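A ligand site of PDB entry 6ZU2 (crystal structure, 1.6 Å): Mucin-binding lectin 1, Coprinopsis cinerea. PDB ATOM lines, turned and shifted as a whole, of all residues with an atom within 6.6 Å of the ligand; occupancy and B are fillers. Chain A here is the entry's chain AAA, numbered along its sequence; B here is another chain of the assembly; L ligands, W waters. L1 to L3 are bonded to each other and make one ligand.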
ATOM      1  N   HIS A   4      26.767  22.769  28.599  1.00  0.00           N
ATOM      2  CA  HIS A   4      26.426  23.034  30.008  1.00  0.00           C
ATOM      3  C   HIS A   4      25.863  24.443  30.098  1.00  0.00           C
ATOM      4  O   HIS A   4      26.205  25.320  29.287  1.00  0.00           O
ATOM      5  CB  HIS A   4      27.607  22.837  30.940  1.00  0.00           C
ATOM      6  CG  HIS A   4      28.112  21.441  30.905  1.00  0.00           C
ATOM      7  ND1 HIS A   4      28.579  20.820  32.032  1.00  0.00           N
ATOM      8  CD2 HIS A   4      28.220  20.541  29.906  1.00  0.00           C
ATOM      9  CE1 HIS A   4      28.955  19.609  31.740  1.00  0.00           C
ATOM     10  NE2 HIS A   4      28.758  19.392  30.451  1.00  0.00           N
ATOM     11  N   LEU A  27      25.832   6.191  22.436  1.00  0.00           N
ATOM     12  CA  LEU A  27      26.005   5.074  23.411  1.00  0.00           C
ATOM     13  C   LEU A  27      25.184   3.849  22.980  1.00  0.00           C
ATOM     14  O   LEU A  27      24.048   3.960  22.472  1.00  0.00           O
ATOM     15  CB  LEU A  27      25.591   5.533  24.809  1.00  0.00           C
ATOM     16  CG  LEU A  27      26.444   6.603  25.482  1.00  0.00           C
ATOM     17  CD1 LEU A  27      25.885   6.994  26.844  1.00  0.00           C
ATOM     18  CD2 LEU A  27      27.902   6.176  25.606  1.00  0.00           C
ATOM     19  N   PHE A  51      22.530  19.586  21.977  1.00  0.00           N
ATOM     20  CA  PHE A  51      22.871  18.151  21.974  1.00  0.00           C
ATOM     21  C   PHE A  51      21.599  17.274  22.129  1.00  0.00           C
ATOM     22  O   PHE A  51      20.509  17.799  22.339  1.00  0.00           O
ATOM     23  CB  PHE A  51      23.870  17.838  23.074  1.00  0.00           C
ATOM     24  CG  PHE A  51      23.347  17.830  24.479  1.00  0.00           C
ATOM     25  CD1 PHE A  51      23.191  19.026  25.137  1.00  0.00           C
ATOM     26  CD2 PHE A  51      23.099  16.640  25.122  1.00  0.00           C
ATOM     27  CE1 PHE A  51      22.795  19.039  26.455  1.00  0.00           C
ATOM     28  CE2 PHE A  51      22.711  16.649  26.460  1.00  0.00           C
ATOM     29  CZ  PHE A  51      22.537  17.842  27.089  1.00  0.00           C
ATOM     30  N   SER A  52      21.776  15.951  22.057  1.00  0.00           N
ATOM     31  CA  SER A  52      20.785  14.892  22.381  1.00  0.00           C
ATOM     32  C   SER A  52      21.409  14.050  23.483  1.00  0.00           C
ATOM     33  O   SER A  52      22.588  13.702  23.341  1.00  0.00           O
ATOM     34  CB  SER A  52      20.430  14.002  21.256  1.00  0.00           C
ATOM     35  OG  SER A  52      19.501  14.614  20.421  1.00  0.00           O
ATOM     36  N   HIS A  53      20.700  13.793  24.578  1.00  0.00           N
ATOM     37  CA  HIS A  53      21.224  12.811  25.558  1.00  0.00           C
ATOM     38  C   HIS A  53      21.567  11.511  24.866  1.00  0.00           C
ATOM     39  O   HIS A  53      20.960  11.130  23.907  1.00  0.00           O
ATOM     40  CB  HIS A  53      20.244  12.614  26.733  1.00  0.00           C
ATOM     41  CG  HIS A  53      20.117  13.809  27.601  1.00  0.00           C
ATOM     42  ND1 HIS A  53      21.095  14.190  28.512  1.00  0.00           N
ATOM     43  CD2 HIS A  53      19.149  14.754  27.708  1.00  0.00           C
ATOM     44  CE1 HIS A  53      20.720  15.279  29.126  1.00  0.00           C
ATOM     45  NE2 HIS A  53      19.523  15.677  28.613  1.00  0.00           N
ATOM     46  N   ASN A  54      22.574  10.838  25.448  1.00  0.00           N
ATOM     47  CA  ASN A  54      23.087   9.519  25.045  1.00  0.00           C
ATOM     48  C   ASN A  54      23.963   9.613  23.794  1.00  0.00           C
ATOM     49  O   ASN A  54      24.314   8.504  23.297  1.00  0.00           O
ATOM     50  CB  ASN A  54      22.003   8.459  24.902  1.00  0.00           C
ATOM     51  CG  ASN A  54      21.044   8.422  26.052  1.00  0.00           C
ATOM     52  OD1 ASN A  54      21.458   8.317  27.213  1.00  0.00           O
ATOM     53  ND2 ASN A  54      19.780   8.654  25.743  1.00  0.00           N
ATOM     54  N   TYR A  55      24.332  10.791  23.344  1.00  0.00           N
ATOM     55  CA  TYR A  55      25.297  10.932  22.209  1.00  0.00           C
ATOM     56  C   TYR A  55      26.523  11.660  22.659  1.00  0.00           C
ATOM     57  O   TYR A  55      26.472  12.539  23.503  1.00  0.00           O
ATOM     58  CB  TYR A  55      24.646  11.627  21.029  1.00  0.00           C
ATOM     59  CG  TYR A  55      23.620  10.800  20.319  1.00  0.00           C
ATOM     60  CD1 TYR A  55      22.283  10.832  20.675  1.00  0.00           C
ATOM     61  CD2 TYR A  55      23.926   9.995  19.225  1.00  0.00           C
ATOM     62  CE1 TYR A  55      21.328  10.106  19.994  1.00  0.00           C
ATOM     63  CE2 TYR A  55      22.998   9.261  18.522  1.00  0.00           C
ATOM     64  CZ  TYR A  55      21.652   9.325  18.885  1.00  0.00           C
ATOM     65  OH  TYR A  55      20.727   8.595  18.211  1.00  0.00           O
ATOM     66  N   THR A  56      27.677  11.344  22.017  1.00  0.00           N
ATOM     67  CA  THR A  56      28.948  11.912  22.515  1.00  0.00           C
ATOM     68  C   THR A  56      29.732  12.738  21.463  1.00  0.00           C
ATOM     69  O   THR A  56      30.704  13.408  21.856  1.00  0.00           O
ATOM     70  CB  THR A  56      29.900  10.829  23.019  1.00  0.00           C
ATOM     71  OG1 THR A  56      30.248  10.064  21.904  1.00  0.00           O
ATOM     72  CG2 THR A  56      29.294   9.970  24.108  1.00  0.00           C
ATOM     73  N   ARG A  57      29.142  12.915  20.290  1.00  0.00           N
ATOM     74  CA  ARG A  57      29.728  13.735  19.209  1.00  0.00           C
ATOM     75  C   ARG A  57      28.603  14.524  18.491  1.00  0.00           C
ATOM     76  O   ARG A  57      27.609  13.941  18.159  1.00  0.00           O
ATOM     77  CB  ARG A  57      30.460  12.865  18.182  1.00  0.00           C
ATOM     78  CG  ARG A  57      31.643  12.016  18.679  1.00  0.00           C
ATOM     79  CD  ARG A  57      32.762  12.923  19.084  1.00  0.00           C
ATOM     80  NE  ARG A  57      33.943  12.192  19.544  1.00  0.00           N
ATOM     81  CZ  ARG A  57      34.214  11.934  20.812  1.00  0.00           C
ATOM     82  NH1 ARG A  57      33.360  12.224  21.762  1.00  0.00           N
ATOM     83  NH2 ARG A  57      35.322  11.263  21.109  1.00  0.00           N
ATOM     84  N   TRP A  93      31.731  15.505  23.410  1.00  0.00           N
ATOM     85  CA  TRP A  93      31.014  15.658  24.701  1.00  0.00           C
ATOM     86  C   TRP A  93      32.041  15.869  25.824  1.00  0.00           C
ATOM     87  O   TRP A  93      32.932  14.997  25.949  1.00  0.00           O
ATOM     88  CB  TRP A  93      30.134  14.426  24.927  1.00  0.00           C
ATOM     89  CG  TRP A  93      29.285  14.519  26.149  1.00  0.00           C
ATOM     90  CD1 TRP A  93      29.394  13.797  27.297  1.00  0.00           C
ATOM     91  CD2 TRP A  93      28.233  15.474  26.364  1.00  0.00           C
ATOM     92  NE1 TRP A  93      28.435  14.206  28.190  1.00  0.00           N
ATOM     93  CE2 TRP A  93      27.700  15.230  27.652  1.00  0.00           C
ATOM     94  CE3 TRP A  93      27.673  16.493  25.576  1.00  0.00           C
ATOM     95  CZ2 TRP A  93      26.648  15.986  28.160  1.00  0.00           C
ATOM     96  CZ3 TRP A  93      26.613  17.205  26.080  1.00  0.00           C
ATOM     97  CH2 TRP A  93      26.126  16.982  27.361  1.00  0.00           C
ATOM     98  N   GLY A  94      31.902  16.915  26.613  1.00  0.00           N
ATOM     99  CA  GLY A  94      32.778  17.192  27.762  1.00  0.00           C
ATOM    100  C   GLY A  94      33.868  18.182  27.387  1.00  0.00           C
ATOM    101  O   GLY A  94      34.431  18.811  28.295  1.00  0.00           O
ATOM    102  N   ARG B  31      17.187   5.438  29.649  1.00  0.00           N
ATOM    103  CA  ARG B  31      16.829   5.991  30.967  1.00  0.00           C
ATOM    104  C   ARG B  31      16.260   7.412  30.772  1.00  0.00           C
ATOM    105  O   ARG B  31      16.851   8.236  30.034  1.00  0.00           O
ATOM    106  CB  ARG B  31      18.081   6.083  31.830  1.00  0.00           C
ATOM    107  CG  ARG B  31      17.880   6.818  33.147  1.00  0.00           C
ATOM    108  CD  ARG B  31      18.219   5.939  34.294  1.00  0.00           C
ATOM    109  NE  ARG B  31      17.962   6.499  35.591  1.00  0.00           N
ATOM    110  CZ  ARG B  31      18.868   6.637  36.534  1.00  0.00           C
ATOM    111  NH1 ARG B  31      20.123   6.321  36.267  1.00  0.00           N
ATOM    112  NH2 ARG B  31      18.528   7.108  37.730  1.00  0.00           N
ATOM    113  N   SER B  32      15.215   7.763  31.530  1.00  0.00           N
ATOM    114  CA  SER B  32      14.672   9.119  31.544  1.00  0.00           C
ATOM    115  C   SER B  32      15.679  10.063  32.189  1.00  0.00           C
ATOM    116  O   SER B  32      16.459   9.633  33.084  1.00  0.00           O
ATOM    117  CB  SER B  32      13.344   9.183  32.240  1.00  0.00           C
ATOM    118  OG  SER B  32      12.418   8.368  31.579  1.00  0.00           O
ATOM    119  N   VAL B  33      15.681  11.331  31.804  1.00  0.00           N
ATOM    120  CA  VAL B  33      16.655  12.315  32.304  1.00  0.00           C
ATOM    121  C   VAL B  33      15.862  13.453  32.893  1.00  0.00           C
ATOM    122  O   VAL B  33      14.808  13.847  32.285  1.00  0.00           O
ATOM    123  CB  VAL B  33      17.534  12.810  31.148  1.00  0.00           C
ATOM    124  CG1 VAL B  33      18.381  13.960  31.637  1.00  0.00           C
ATOM    125  CG2 VAL B  33      18.295  11.660  30.533  1.00  0.00           C
ATOM    126  N   TYR B  55      13.707   9.821  22.211  1.00  0.00           N
ATOM    127  CA  TYR B  55      12.701   9.989  23.276  1.00  0.00           C
ATOM    128  C   TYR B  55      11.376  10.455  22.726  1.00  0.00           C
ATOM    129  O   TYR B  55      11.382  11.194  21.726  1.00  0.00           O
ATOM    130  CB  TYR B  55      13.235  10.937  24.334  1.00  0.00           C
ATOM    131  CG  TYR B  55      14.366  10.406  25.167  1.00  0.00           C
ATOM    132  CD1 TYR B  55      15.689  10.605  24.789  1.00  0.00           C
ATOM    133  CD2 TYR B  55      14.121   9.745  26.343  1.00  0.00           C
ATOM    134  CE1 TYR B  55      16.727  10.165  25.588  1.00  0.00           C
ATOM    135  CE2 TYR B  55      15.144   9.269  27.128  1.00  0.00           C
ATOM    136  CZ  TYR B  55      16.452   9.495  26.768  1.00  0.00           C
ATOM    137  OH  TYR B  55      17.463   9.062  27.579  1.00  0.00           O
ATOM    138  N   VAL B 111      17.438  10.014  35.710  1.00  0.00           N
ATOM    139  CA  VAL B 111      18.817  10.373  36.157  1.00  0.00           C
ATOM    140  C   VAL B 111      18.939  11.877  36.193  1.00  0.00           C
ATOM    141  O   VAL B 111      18.481  12.578  35.257  1.00  0.00           O
ATOM    142  CB  VAL B 111      19.911   9.754  35.280  1.00  0.00           C
ATOM    143  CG1 VAL B 111      19.838  10.174  33.836  1.00  0.00           C
ATOM    144  CG2 VAL B 111      21.278  10.067  35.876  1.00  0.00           C
ATOM    145  N   ARG B 113      20.487  15.413  35.700  1.00  0.00           N
ATOM    146  CA  ARG B 113      21.455  16.085  34.794  1.00  0.00           C
ATOM    147  C   ARG B 113      21.300  17.602  34.968  1.00  0.00           C
ATOM    148  O   ARG B 113      21.270  18.376  33.967  1.00  0.00           O
ATOM    149  CB  ARG B 113      21.281  15.629  33.354  1.00  0.00           C
ATOM    150  CG  ARG B 113      21.525  14.147  33.135  1.00  0.00           C
ATOM    151  CD  ARG B 113      22.908  13.738  33.558  1.00  0.00           C
ATOM    152  NE  ARG B 113      23.129  12.370  33.122  1.00  0.00           N
ATOM    153  CZ  ARG B 113      23.868  11.416  33.741  1.00  0.00           C
ATOM    154  NH1 ARG B 113      24.462  11.691  34.879  1.00  0.00           N
ATOM    155  NH2 ARG B 113      23.958  10.231  33.211  1.00  0.00           N
ATOM    156  N   VAL B 116      22.865  20.476  32.731  1.00  0.00           N
ATOM    157  CA  VAL B 116      23.350  19.787  31.520  1.00  0.00           C
ATOM    158  C   VAL B 116      22.206  19.029  30.883  1.00  0.00           C
ATOM    159  O   VAL B 116      22.308  17.837  30.637  1.00  0.00           O
ATOM    160  CB  VAL B 116      24.540  18.840  31.777  1.00  0.00           C
ATOM    161  CG1 VAL B 116      25.258  18.540  30.477  1.00  0.00           C
ATOM    162  CG2 VAL B 116      25.495  19.338  32.846  1.00  0.00           C
HETATM  163  C1  LIG L   1      30.565  11.020  30.163  1.00  0.00           C
HETATM  164  C2  LIG L   1      29.070  10.626  30.180  1.00  0.00           C
HETATM  165  C3  LIG L   1      28.905   9.142  29.993  1.00  0.00           C
HETATM  166  C4  LIG L   1      29.665   8.777  28.749  1.00  0.00           C
HETATM  167  C5  LIG L   1      31.077   9.349  28.613  1.00  0.00           C
HETATM  168  C6  LIG L   1      31.553   9.127  27.174  1.00  0.00           C
HETATM  169  C7  LIG L   1      27.711  12.131  31.527  1.00  0.00           C
HETATM  170  C8  LIG L   1      27.235  12.364  32.944  1.00  0.00           C
HETATM  171  N1  LIG L   1      28.398  11.023  31.361  1.00  0.00           N
HETATM  172  O1  LIG L   1      30.773  12.408  30.298  1.00  0.00           O
HETATM  173  O2  LIG L   1      27.521   8.767  29.712  1.00  0.00           O
HETATM  174  O3  LIG L   1      29.681   7.361  28.594  1.00  0.00           O
HETATM  175  O4  LIG L   1      31.075  10.748  28.900  1.00  0.00           O
HETATM  176  O5  LIG L   1      32.234  10.287  26.684  1.00  0.00           O
HETATM  177  O6  LIG L   1      27.496  12.992  30.634  1.00  0.00           O
HETATM  178  C1  LG2 L   2      26.813   8.089  30.725  1.00  0.00           C
HETATM  179  C2  LG2 L   2      25.333   7.943  30.320  1.00  0.00           C
HETATM  180  C3  LG2 L   2      24.582   7.166  31.392  1.00  0.00           C
HETATM  181  C4  LG2 L   2      25.269   5.809  31.667  1.00  0.00           C
HETATM  182  C5  LG2 L   2      26.754   6.043  31.907  1.00  0.00           C
HETATM  183  C6  LG2 L   2      27.565   4.744  31.959  1.00  0.00           C
HETATM  184  O1  LG2 L   2      24.756   9.250  30.304  1.00  0.00           O
HETATM  185  O2  LG2 L   2      23.215   6.867  30.966  1.00  0.00           O
HETATM  186  O3  LG2 L   2      25.229   5.027  30.514  1.00  0.00           O
HETATM  187  O4  LG2 L   2      27.344   6.733  30.834  1.00  0.00           O
HETATM  188  O5  LG2 L   2      28.756   5.101  32.679  1.00  0.00           O
HETATM  189  C1  LG3 L   3      23.931   9.581  29.153  1.00  0.00           C
HETATM  190  C2  LG3 L   3      23.145  10.807  29.536  1.00  0.00           C
HETATM  191  C3  LG3 L   3      23.968  12.056  29.750  1.00  0.00           C
HETATM  192  C4  LG3 L   3      24.854  12.270  28.531  1.00  0.00           C
HETATM  193  C5  LG3 L   3      25.571  11.001  28.213  1.00  0.00           C
HETATM  194  C6  LG3 L   3      26.354  11.087  26.901  1.00  0.00           C
HETATM  195  O1  LG3 L   3      22.418  10.621  30.785  1.00  0.00           O
HETATM  196  O2  LG3 L   3      23.207  13.161  30.087  1.00  0.00           O
HETATM  197  O3  LG3 L   3      23.916  12.599  27.423  1.00  0.00           O
HETATM  198  O4  LG3 L   3      24.769   9.853  28.013  1.00  0.00           O
HETATM  199  O   HOH W   1      33.741  12.422  24.396  1.00  0.00           O
HETATM  200  O   HOH W   2      23.680   2.875  31.073  1.00  0.00           O
HETATM  201  O   HOH W   3      21.986   6.474  33.718  1.00  0.00           O
HETATM  202  O   HOH W   4      22.255   6.039  28.746  1.00  0.00           O
HETATM  203  O   HOH W   5      24.152  15.616  30.613  1.00  0.00           O
HETATM  204  O   HOH W   6      25.064  14.015  25.427  1.00  0.00           O
HETATM  205  O   HOH W   7      20.258   9.125  29.729  1.00  0.00           O
HETATM  206  O   HOH W   8      26.576  15.459  31.756  1.00  0.00           O
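Water W4 bridges O2 of LG2 L2 and OD1 of Asn 54. Water W5 bridges an oxygen (O2) of LG3 L3 (2.7 Å) and the backbone carbonyl oxygen (O) of Val 116 of chain B (2.9 Å). Water W6 lies within hydrogen-bond range of O3 of LG3 L3 (2.7 Å), O of Tyr 55 of chain A (2.8 Å) and O of Ser 52 (3.3 Å). Water W7 lies within hydrogen-bond range of an oxygen (O1) of LG3 L3 and the side-chain amide oxygen (OD1) of Asn 54. Water W3 lies within hydrogen-bond range of an oxygen (O2) of LG2 L2 and the guanidinium group of Arg 31 of chain B. Water W1 lies within hydrogen-bond range of the guanidinium group (NH1) of Arg 57, the backbone carbonyl oxygen (O) of Trp 93 and an oxygen (O5) of LIG L1.
CD1 of Leu 27 touches O4 of LG3 L3, at 3.3 Å. O of Tyr 55 of chain A touches C6 of LG3 L3, 3.7 Å away. CG2 of Thr 56 touches C6 of LIG L1 (3.9 Å). Hydrophobic or aromatic side chains within 4 Å of the ligand: Leu 27, His 53 and Trp 93.
A ring nitrogen (ND1) of His 53 is in hydrogen-bond range of an oxygen (O2) of LG3 L3. The indole nitrogen (NE1) of Trp 93 lies within hydrogen-bond range of an oxygen (O6) of LIG L1 (2.9 Å). O1 of LG3 L3 is in hydrogen-bond range of NH2 of Arg 113 of chain B (2.9 Å). N of Asn 54 lies within hydrogen-bond range of O3 of LG3 L3 (3.0 Å).
The backbone NH (N) of Trp 93 is in hydrogen-bond range of the backbone carbonyl oxygen (O) of Thr 56, at 2.8 Å. The backbone NH (N) of Leu 27 is in hydrogen-bond range of the backbone carbonyl oxygen (O) of Asn 54. OH of Tyr 55 of chain B lies within hydrogen-bond range of ND2 of Asn 54, 3.0 Å away.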
